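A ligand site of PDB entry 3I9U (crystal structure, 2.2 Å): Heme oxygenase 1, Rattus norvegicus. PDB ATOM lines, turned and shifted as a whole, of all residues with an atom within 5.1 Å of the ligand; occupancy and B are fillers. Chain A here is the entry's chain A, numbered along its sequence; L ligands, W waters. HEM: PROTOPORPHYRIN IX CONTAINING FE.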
ATOM      1  N   SER A  14     -21.241 -10.356  16.595  1.00  0.00           N
ATOM      2  CA  SER A  14     -21.298 -11.670  17.325  1.00  0.00           C
ATOM      3  C   SER A  14     -21.205 -11.481  18.858  1.00  0.00           C
ATOM      4  O   SER A  14     -21.824 -12.237  19.604  1.00  0.00           O
ATOM      5  CB  SER A  14     -20.198 -12.633  16.849  1.00  0.00           C
ATOM      6  OG  SER A  14     -18.944 -12.116  17.253  1.00  0.00           O
ATOM      7  N   LYS A  18     -24.273 -12.021  21.707  1.00  0.00           N
ATOM      8  CA  LYS A  18     -24.007 -12.866  22.861  1.00  0.00           C
ATOM      9  C   LYS A  18     -24.402 -12.102  24.155  1.00  0.00           C
ATOM     10  O   LYS A  18     -25.116 -12.655  24.972  1.00  0.00           O
ATOM     11  CB  LYS A  18     -22.519 -13.345  22.896  1.00  0.00           C
ATOM     12  CG  LYS A  18     -22.114 -14.274  24.143  1.00  0.00           C
ATOM     13  CD  LYS A  18     -20.582 -14.503  24.193  1.00  0.00           C
ATOM     14  CE  LYS A  18     -20.175 -15.541  25.239  1.00  0.00           C
ATOM     15  NZ  LYS A  18     -20.712 -16.913  24.907  1.00  0.00           N
ATOM     16  N   HIS A  25     -31.137 -16.085  27.778  1.00  0.00           N
ATOM     17  CA  HIS A  25     -30.673 -17.502  27.683  1.00  0.00           C
ATOM     18  C   HIS A  25     -30.833 -18.189  29.062  1.00  0.00           C
ATOM     19  O   HIS A  25     -31.362 -19.312  29.188  1.00  0.00           O
ATOM     20  CB  HIS A  25     -29.237 -17.578  27.217  1.00  0.00           C
ATOM     21  CG  HIS A  25     -28.779 -18.975  26.987  1.00  0.00           C
ATOM     22  ND1 HIS A  25     -28.668 -19.900  28.001  1.00  0.00           N
ATOM     23  CD2 HIS A  25     -28.516 -19.639  25.841  1.00  0.00           C
ATOM     24  CE1 HIS A  25     -28.322 -21.065  27.503  1.00  0.00           C
ATOM     25  NE2 HIS A  25     -28.209 -20.938  26.189  1.00  0.00           N
ATOM     26  N   ALA A  28     -34.475 -19.004  29.542  1.00  0.00           N
ATOM     27  CA  ALA A  28     -34.849 -20.095  28.655  1.00  0.00           C
ATOM     28  C   ALA A  28     -34.365 -21.445  29.165  1.00  0.00           C
ATOM     29  O   ALA A  28     -35.125 -22.379  29.146  1.00  0.00           O
ATOM     30  CB  ALA A  28     -34.335 -19.852  27.159  1.00  0.00           C
ATOM     31  N   GLU A  29     -33.104 -21.536  29.558  1.00  0.00           N
ATOM     32  CA  GLU A  29     -32.502 -22.741  30.125  1.00  0.00           C
ATOM     33  C   GLU A  29     -33.292 -23.211  31.343  1.00  0.00           C
ATOM     34  O   GLU A  29     -33.210 -24.426  31.668  1.00  0.00           O
ATOM     35  CB  GLU A  29     -31.169 -22.382  30.784  1.00  0.00           C
ATOM     36  CG  GLU A  29     -29.979 -22.510  29.974  1.00  0.00           C
ATOM     37  CD  GLU A  29     -28.806 -22.025  30.760  1.00  0.00           C
ATOM     38  OE1 GLU A  29     -28.449 -20.795  30.725  1.00  0.00           O
ATOM     39  OE2 GLU A  29     -28.213 -22.884  31.416  1.00  0.00           O
ATOM     40  N   MET A  34     -37.364 -27.192  29.720  1.00  0.00           N
ATOM     41  CA  MET A  34     -35.910 -27.404  29.609  1.00  0.00           C
ATOM     42  C   MET A  34     -35.254 -27.922  30.889  1.00  0.00           C
ATOM     43  O   MET A  34     -34.304 -28.727  30.814  1.00  0.00           O
ATOM     44  CB  MET A  34     -35.207 -26.158  29.078  1.00  0.00           C
ATOM     45  CG  MET A  34     -35.569 -25.847  27.645  1.00  0.00           C
ATOM     46  SD  MET A  34     -34.892 -27.155  26.558  1.00  0.00           S
ATOM     47  CE  MET A  34     -36.076 -27.115  25.282  1.00  0.00           C
ATOM     48  N   GLN A  38     -33.197 -31.401  30.871  1.00  0.00           N
ATOM     49  CA  GLN A  38     -31.827 -31.427  31.326  1.00  0.00           C
ATOM     50  C   GLN A  38     -31.610 -32.425  32.380  1.00  0.00           C
ATOM     51  O   GLN A  38     -30.484 -32.888  32.502  1.00  0.00           O
ATOM     52  CB  GLN A  38     -31.493 -30.117  31.962  1.00  0.00           C
ATOM     53  CG  GLN A  38     -31.010 -29.160  31.025  1.00  0.00           C
ATOM     54  CD  GLN A  38     -30.408 -27.974  31.715  1.00  0.00           C
ATOM     55  OE1 GLN A  38     -29.188 -27.922  31.866  1.00  0.00           O
ATOM     56  NE2 GLN A  38     -31.244 -27.000  32.139  1.00  0.00           N
ATOM     57  N   TYR A 134     -28.832 -16.972  14.052  1.00  0.00           N
ATOM     58  CA  TYR A 134     -27.977 -16.958  15.214  1.00  0.00           C
ATOM     59  C   TYR A 134     -28.662 -17.699  16.361  1.00  0.00           C
ATOM     60  O   TYR A 134     -28.060 -18.641  16.951  1.00  0.00           O
ATOM     61  CB  TYR A 134     -27.664 -15.496  15.638  1.00  0.00           C
ATOM     62  CG  TYR A 134     -27.092 -15.421  17.031  1.00  0.00           C
ATOM     63  CD1 TYR A 134     -25.733 -15.691  17.280  1.00  0.00           C
ATOM     64  CD2 TYR A 134     -27.916 -15.102  18.118  1.00  0.00           C
ATOM     65  CE1 TYR A 134     -25.188 -15.656  18.577  1.00  0.00           C
ATOM     66  CE2 TYR A 134     -27.387 -15.073  19.466  1.00  0.00           C
ATOM     67  CZ  TYR A 134     -26.043 -15.308  19.675  1.00  0.00           C
ATOM     68  OH  TYR A 134     -25.548 -15.275  20.982  1.00  0.00           O
ATOM     69  N   THR A 135     -29.895 -17.306  16.710  1.00  0.00           N
ATOM     70  CA  THR A 135     -30.571 -17.887  17.900  1.00  0.00           C
ATOM     71  C   THR A 135     -30.701 -19.432  17.823  1.00  0.00           C
ATOM     72  O   THR A 135     -30.459 -20.129  18.811  1.00  0.00           O
ATOM     73  CB  THR A 135     -31.937 -17.200  18.139  1.00  0.00           C
ATOM     74  OG1 THR A 135     -31.714 -15.806  18.454  1.00  0.00           O
ATOM     75  CG2 THR A 135     -32.857 -17.912  19.273  1.00  0.00           C
ATOM     76  N   ARG A 136     -31.088 -19.948  16.663  1.00  0.00           N
ATOM     77  CA  ARG A 136     -31.274 -21.368  16.443  1.00  0.00           C
ATOM     78  C   ARG A 136     -29.918 -22.066  16.214  1.00  0.00           C
ATOM     79  O   ARG A 136     -29.506 -22.882  17.008  1.00  0.00           O
ATOM     80  CB  ARG A 136     -32.260 -21.628  15.267  1.00  0.00           C
ATOM     81  CG  ARG A 136     -33.783 -21.452  15.639  1.00  0.00           C
ATOM     82  CD  ARG A 136     -34.263 -22.145  16.994  1.00  0.00           C
ATOM     83  NE  ARG A 136     -33.580 -23.415  17.216  1.00  0.00           N
ATOM     84  CZ  ARG A 136     -33.757 -24.241  18.265  1.00  0.00           C
ATOM     85  NH1 ARG A 136     -34.646 -23.934  19.194  1.00  0.00           N
ATOM     86  NH2 ARG A 136     -33.039 -25.401  18.371  1.00  0.00           N
ATOM     87  N   LEU A 138     -26.527 -21.342  16.298  1.00  0.00           N
ATOM     88  CA  LEU A 138     -25.418 -21.313  17.241  1.00  0.00           C
ATOM     89  C   LEU A 138     -25.698 -22.070  18.530  1.00  0.00           C
ATOM     90  O   LEU A 138     -24.742 -22.598  19.159  1.00  0.00           O
ATOM     91  CB  LEU A 138     -24.944 -19.878  17.558  1.00  0.00           C
ATOM     92  CG  LEU A 138     -24.011 -19.173  16.525  1.00  0.00           C
ATOM     93  CD1 LEU A 138     -22.933 -18.378  17.204  1.00  0.00           C
ATOM     94  CD2 LEU A 138     -23.311 -20.104  15.524  1.00  0.00           C
ATOM     95  N   GLY A 139     -26.962 -22.144  18.962  1.00  0.00           N
ATOM     96  CA  GLY A 139     -27.222 -22.953  20.114  1.00  0.00           C
ATOM     97  C   GLY A 139     -27.154 -24.399  19.662  1.00  0.00           C
ATOM     98  O   GLY A 139     -26.636 -25.292  20.404  1.00  0.00           O
ATOM     99  N   SER A 142     -23.914 -25.670  20.145  1.00  0.00           N
ATOM    100  CA  SER A 142     -23.406 -25.501  21.516  1.00  0.00           C
ATOM    101  C   SER A 142     -24.101 -26.452  22.504  1.00  0.00           C
ATOM    102  O   SER A 142     -23.848 -27.667  22.537  1.00  0.00           O
ATOM    103  CB  SER A 142     -23.755 -24.108  21.964  1.00  0.00           C
ATOM    104  OG  SER A 142     -23.011 -23.250  21.221  1.00  0.00           O
ATOM    105  N   GLY A 143     -25.000 -25.857  23.261  1.00  0.00           N
ATOM    106  CA  GLY A 143     -25.854 -26.585  24.179  1.00  0.00           C
ATOM    107  C   GLY A 143     -26.709 -27.670  23.551  1.00  0.00           C
ATOM    108  O   GLY A 143     -27.005 -28.665  24.203  1.00  0.00           O
ATOM    109  N   VAL A 146     -25.169 -30.886  24.041  1.00  0.00           N
ATOM    110  CA  VAL A 146     -25.356 -31.440  25.406  1.00  0.00           C
ATOM    111  C   VAL A 146     -26.765 -32.075  25.507  1.00  0.00           C
ATOM    112  O   VAL A 146     -26.905 -33.197  25.983  1.00  0.00           O
ATOM    113  CB  VAL A 146     -25.132 -30.347  26.469  1.00  0.00           C
ATOM    114  CG1 VAL A 146     -25.329 -30.900  27.921  1.00  0.00           C
ATOM    115  CG2 VAL A 146     -23.696 -29.620  26.266  1.00  0.00           C
ATOM    116  N   LEU A 147     -27.798 -31.408  25.021  1.00  0.00           N
ATOM    117  CA  LEU A 147     -29.142 -31.987  25.095  1.00  0.00           C
ATOM    118  C   LEU A 147     -29.244 -33.294  24.312  1.00  0.00           C
ATOM    119  O   LEU A 147     -29.948 -34.200  24.731  1.00  0.00           O
ATOM    120  CB  LEU A 147     -30.219 -31.003  24.608  1.00  0.00           C
ATOM    121  CG  LEU A 147     -30.340 -29.695  25.415  1.00  0.00           C
ATOM    122  CD1 LEU A 147     -31.317 -28.809  24.705  1.00  0.00           C
ATOM    123  CD2 LEU A 147     -30.850 -30.006  26.804  1.00  0.00           C
ATOM    124  N   LYS A 179     -18.707 -22.660  14.643  1.00  0.00           N
ATOM    125  CA  LYS A 179     -19.245 -21.512  15.358  1.00  0.00           C
ATOM    126  C   LYS A 179     -18.347 -20.296  15.259  1.00  0.00           C
ATOM    127  O   LYS A 179     -18.840 -19.162  15.124  1.00  0.00           O
ATOM    128  CB  LYS A 179     -19.379 -21.830  16.827  1.00  0.00           C
ATOM    129  CG  LYS A 179     -20.701 -22.207  17.321  1.00  0.00           C
ATOM    130  CD  LYS A 179     -20.735 -21.918  18.866  1.00  0.00           C
ATOM    131  CE  LYS A 179     -19.894 -22.933  19.702  1.00  0.00           C
ATOM    132  NZ  LYS A 179     -19.719 -22.244  21.031  1.00  0.00           N
ATOM    133  N   ARG A 183     -19.251 -16.785  13.506  1.00  0.00           N
ATOM    134  CA  ARG A 183     -19.174 -15.533  14.210  1.00  0.00           C
ATOM    135  C   ARG A 183     -18.386 -14.536  13.384  1.00  0.00           C
ATOM    136  O   ARG A 183     -18.805 -13.382  13.213  1.00  0.00           O
ATOM    137  CB  ARG A 183     -18.510 -15.721  15.558  1.00  0.00           C
ATOM    138  CG  ARG A 183     -19.402 -16.419  16.599  1.00  0.00           C
ATOM    139  CD  ARG A 183     -18.756 -16.155  17.946  1.00  0.00           C
ATOM    140  NE  ARG A 183     -19.411 -16.866  19.007  1.00  0.00           N
ATOM    141  CZ  ARG A 183     -18.939 -17.995  19.534  1.00  0.00           C
ATOM    142  NH1 ARG A 183     -17.823 -18.544  19.050  1.00  0.00           N
ATOM    143  NH2 ARG A 183     -19.615 -18.586  20.519  1.00  0.00           N
ATOM    144  N   PHE A 207     -35.642 -15.562  21.233  1.00  0.00           N
ATOM    145  CA  PHE A 207     -35.545 -16.363  22.462  1.00  0.00           C
ATOM    146  C   PHE A 207     -36.894 -16.475  23.138  1.00  0.00           C
ATOM    147  O   PHE A 207     -37.266 -17.574  23.535  1.00  0.00           O
ATOM    148  CB  PHE A 207     -34.567 -15.773  23.433  1.00  0.00           C
ATOM    149  CG  PHE A 207     -33.167 -16.331  23.305  1.00  0.00           C
ATOM    150  CD1 PHE A 207     -32.269 -15.774  22.408  1.00  0.00           C
ATOM    151  CD2 PHE A 207     -32.757 -17.421  24.100  1.00  0.00           C
ATOM    152  CE1 PHE A 207     -30.964 -16.268  22.318  1.00  0.00           C
ATOM    153  CE2 PHE A 207     -31.451 -17.922  24.048  1.00  0.00           C
ATOM    154  CZ  PHE A 207     -30.541 -17.354  23.166  1.00  0.00           C
ATOM    155  N   ASN A 210     -39.082 -18.996  21.614  1.00  0.00           N
ATOM    156  CA  ASN A 210     -38.702 -20.337  22.045  1.00  0.00           C
ATOM    157  C   ASN A 210     -39.223 -20.573  23.455  1.00  0.00           C
ATOM    158  O   ASN A 210     -39.792 -21.634  23.729  1.00  0.00           O
ATOM    159  CB  ASN A 210     -37.166 -20.494  22.020  1.00  0.00           C
ATOM    160  CG  ASN A 210     -36.639 -20.812  20.620  1.00  0.00           C
ATOM    161  OD1 ASN A 210     -36.753 -21.944  20.165  1.00  0.00           O
ATOM    162  ND2 ASN A 210     -36.148 -19.786  19.911  1.00  0.00           N
ATOM    163  N   PHE A 214     -41.806 -23.547  24.709  1.00  0.00           N
ATOM    164  CA  PHE A 214     -41.586 -24.441  25.864  1.00  0.00           C
ATOM    165  C   PHE A 214     -42.698 -24.389  26.884  1.00  0.00           C
ATOM    166  O   PHE A 214     -43.116 -25.441  27.372  1.00  0.00           O
ATOM    167  CB  PHE A 214     -40.260 -24.115  26.586  1.00  0.00           C
ATOM    168  CG  PHE A 214     -39.050 -24.187  25.679  1.00  0.00           C
ATOM    169  CD1 PHE A 214     -39.038 -25.073  24.590  1.00  0.00           C
ATOM    170  CD2 PHE A 214     -37.921 -23.373  25.918  1.00  0.00           C
ATOM    171  CE1 PHE A 214     -37.947 -25.148  23.692  1.00  0.00           C
ATOM    172  CE2 PHE A 214     -36.819 -23.444  25.047  1.00  0.00           C
ATOM    173  CZ  PHE A 214     -36.847 -24.338  23.917  1.00  0.00           C
HETATM  174  CHA HEM L   1     -24.966 -21.280  23.880  1.00  0.00           C
HETATM  175  CHB HEM L   1     -26.612 -24.589  27.053  1.00  0.00           C
HETATM  176  CHC HEM L   1     -31.217 -23.447  25.938  1.00  0.00           C
HETATM  177  CHD HEM L   1     -29.488 -20.715  22.324  1.00  0.00           C
HETATM  178  C1A HEM L   1     -25.022 -22.276  24.839  1.00  0.00           C
HETATM  179  C2A HEM L   1     -23.891 -22.954  25.458  1.00  0.00           C
HETATM  180  C3A HEM L   1     -24.350 -23.825  26.340  1.00  0.00           C
HETATM  181  C4A HEM L   1     -25.784 -23.758  26.313  1.00  0.00           C
HETATM  182  CMA HEM L   1     -23.509 -24.798  27.245  1.00  0.00           C
HETATM  183  CAA HEM L   1     -22.396 -22.639  25.185  1.00  0.00           C
HETATM  184  CBA HEM L   1     -22.165 -21.433  26.107  1.00  0.00           C
HETATM  185  CGA HEM L   1     -20.740 -20.906  26.111  1.00  0.00           C
HETATM  186  O1A HEM L   1     -19.767 -21.719  26.235  1.00  0.00           O
HETATM  187  O2A HEM L   1     -20.568 -19.656  26.034  1.00  0.00           O
HETATM  188  C1B HEM L   1     -28.006 -24.641  26.986  1.00  0.00           C
HETATM  189  C2B HEM L   1     -28.885 -25.589  27.706  1.00  0.00           C
HETATM  190  C3B HEM L   1     -30.140 -25.229  27.372  1.00  0.00           C
HETATM  191  C4B HEM L   1     -30.100 -24.078  26.468  1.00  0.00           C
HETATM  192  CMB HEM L   1     -28.407 -26.771  28.630  1.00  0.00           C
HETATM  193  CAB HEM L   1     -31.477 -25.848  27.795  1.00  0.00           C
HETATM  194  CBB HEM L   1     -31.681 -26.123  29.078  1.00  0.00           C
HETATM  195  C1C HEM L   1     -31.181 -22.609  24.871  1.00  0.00           C
HETATM  196  C2C HEM L   1     -32.305 -22.071  24.108  1.00  0.00           C
HETATM  197  C3C HEM L   1     -31.743 -21.348  23.122  1.00  0.00           C
HETATM  198  C4C HEM L   1     -30.313 -21.380  23.206  1.00  0.00           C
HETATM  199  CMC HEM L   1     -33.822 -22.286  24.366  1.00  0.00           C
HETATM  200  CAC HEM L   1     -32.412 -20.502  22.026  1.00  0.00           C
HETATM  201  CBC HEM L   1     -33.587 -20.848  21.560  1.00  0.00           C
HETATM  202  C1D HEM L   1     -28.141 -20.530  22.366  1.00  0.00           C
HETATM  203  C2D HEM L   1     -27.327 -19.669  21.497  1.00  0.00           C
HETATM  204  C3D HEM L   1     -25.929 -19.857  22.033  1.00  0.00           C
HETATM  205  C4D HEM L   1     -26.021 -20.793  23.130  1.00  0.00           C
HETATM  206  CMD HEM L   1     -27.771 -18.806  20.316  1.00  0.00           C
HETATM  207  CAD HEM L   1     -24.630 -19.243  21.499  1.00  0.00           C
HETATM  208  CBD HEM L   1     -24.237 -18.104  22.430  1.00  0.00           C
HETATM  209  CGD HEM L   1     -23.043 -17.500  21.719  1.00  0.00           C
HETATM  210  O1D HEM L   1     -23.157 -16.359  21.200  1.00  0.00           O
HETATM  211  O2D HEM L   1     -21.982 -18.176  21.644  1.00  0.00           O
HETATM  212  NA  HEM L   1     -26.155 -22.782  25.383  1.00  0.00           N
HETATM  213  NB  HEM L   1     -28.792 -23.743  26.255  1.00  0.00           N
HETATM  214  NC  HEM L   1     -29.997 -22.179  24.293  1.00  0.00           N
HETATM  215  ND  HEM L   1     -27.331 -21.136  23.298  1.00  0.00           N
HETATM  216 FE   HEM L   1     -28.071 -22.420  24.790  1.00  0.00          FE
HETATM  217  O   HOH W   1     -21.532 -15.074  19.747  1.00  0.00           O
HETATM  218  O   HOH W   2     -21.465 -20.530  22.421  1.00  0.00           O
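An oxygen (O2A) of the ligand lies within salt-bridge range of the side-chain amino group of Lys 18 (3.0 Å). O1D of the ligand lies within hydrogen-bond range of OH of Tyr 134 (2.6 Å). NE2 of His 25 is bound to FE of the ligand, 2.0 Å away. O2D of the ligand lies within salt-bridge range of NH2 of Arg 183.
O of Glu 29 lies within hydrogen-bond range of NE2 of Gln 38 (3.3 Å). The side-chain amide oxygen of Asn 210 is in hydrogen-bond range of the guanidinium group of Arg 136 (3.1 Å). OG of Ser 142 sits at hydrogen-bond distance from O of Leu 138. OG of Ser 142 is in hydrogen-bond range of NZ of Lys 179 (3.4 Å). OE1 of Glu 29 lies within hydrogen-bond range of ND1 of His 25.
Merely in contact with the ligand: Ala 28, Glu 29, Met 34, Gln 38, Thr 135, Gly 139, Ser 142, Gly 143, Phe 207, Asn 210 and Phe 214. Hydrophobic or aromatic side chains that line the ligand: His 25, Ala 28, Met 34, Tyr 134, Phe 207 and Phe 214. 15 residues have an atom within 4 Å of the ligand: Lys 18, His 25, Ala 28, Glu 29, Met 34, Gln 38, Tyr 134, Thr 135, Gly 139, Ser 142, Gly 143, Arg 183, Phe 207, Asn 210 and Phe 214. The nearest printed residue that does not touch the ligand is Leu 138 (4.004 Å).
Water W1 lies within hydrogen-bond range of O1D of the ligand (2.5 Å), O of Ser 14 (2.9 Å) and NE of Arg 183 (2.9 Å). Water W2 lies within hydrogen-bond range of O2D of the ligand (2.5 Å), NZ of Lys 179 (2.8 Å), NH2 of Arg 183 (3.3 Å) and OG of Ser 142 (3.4 Å).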
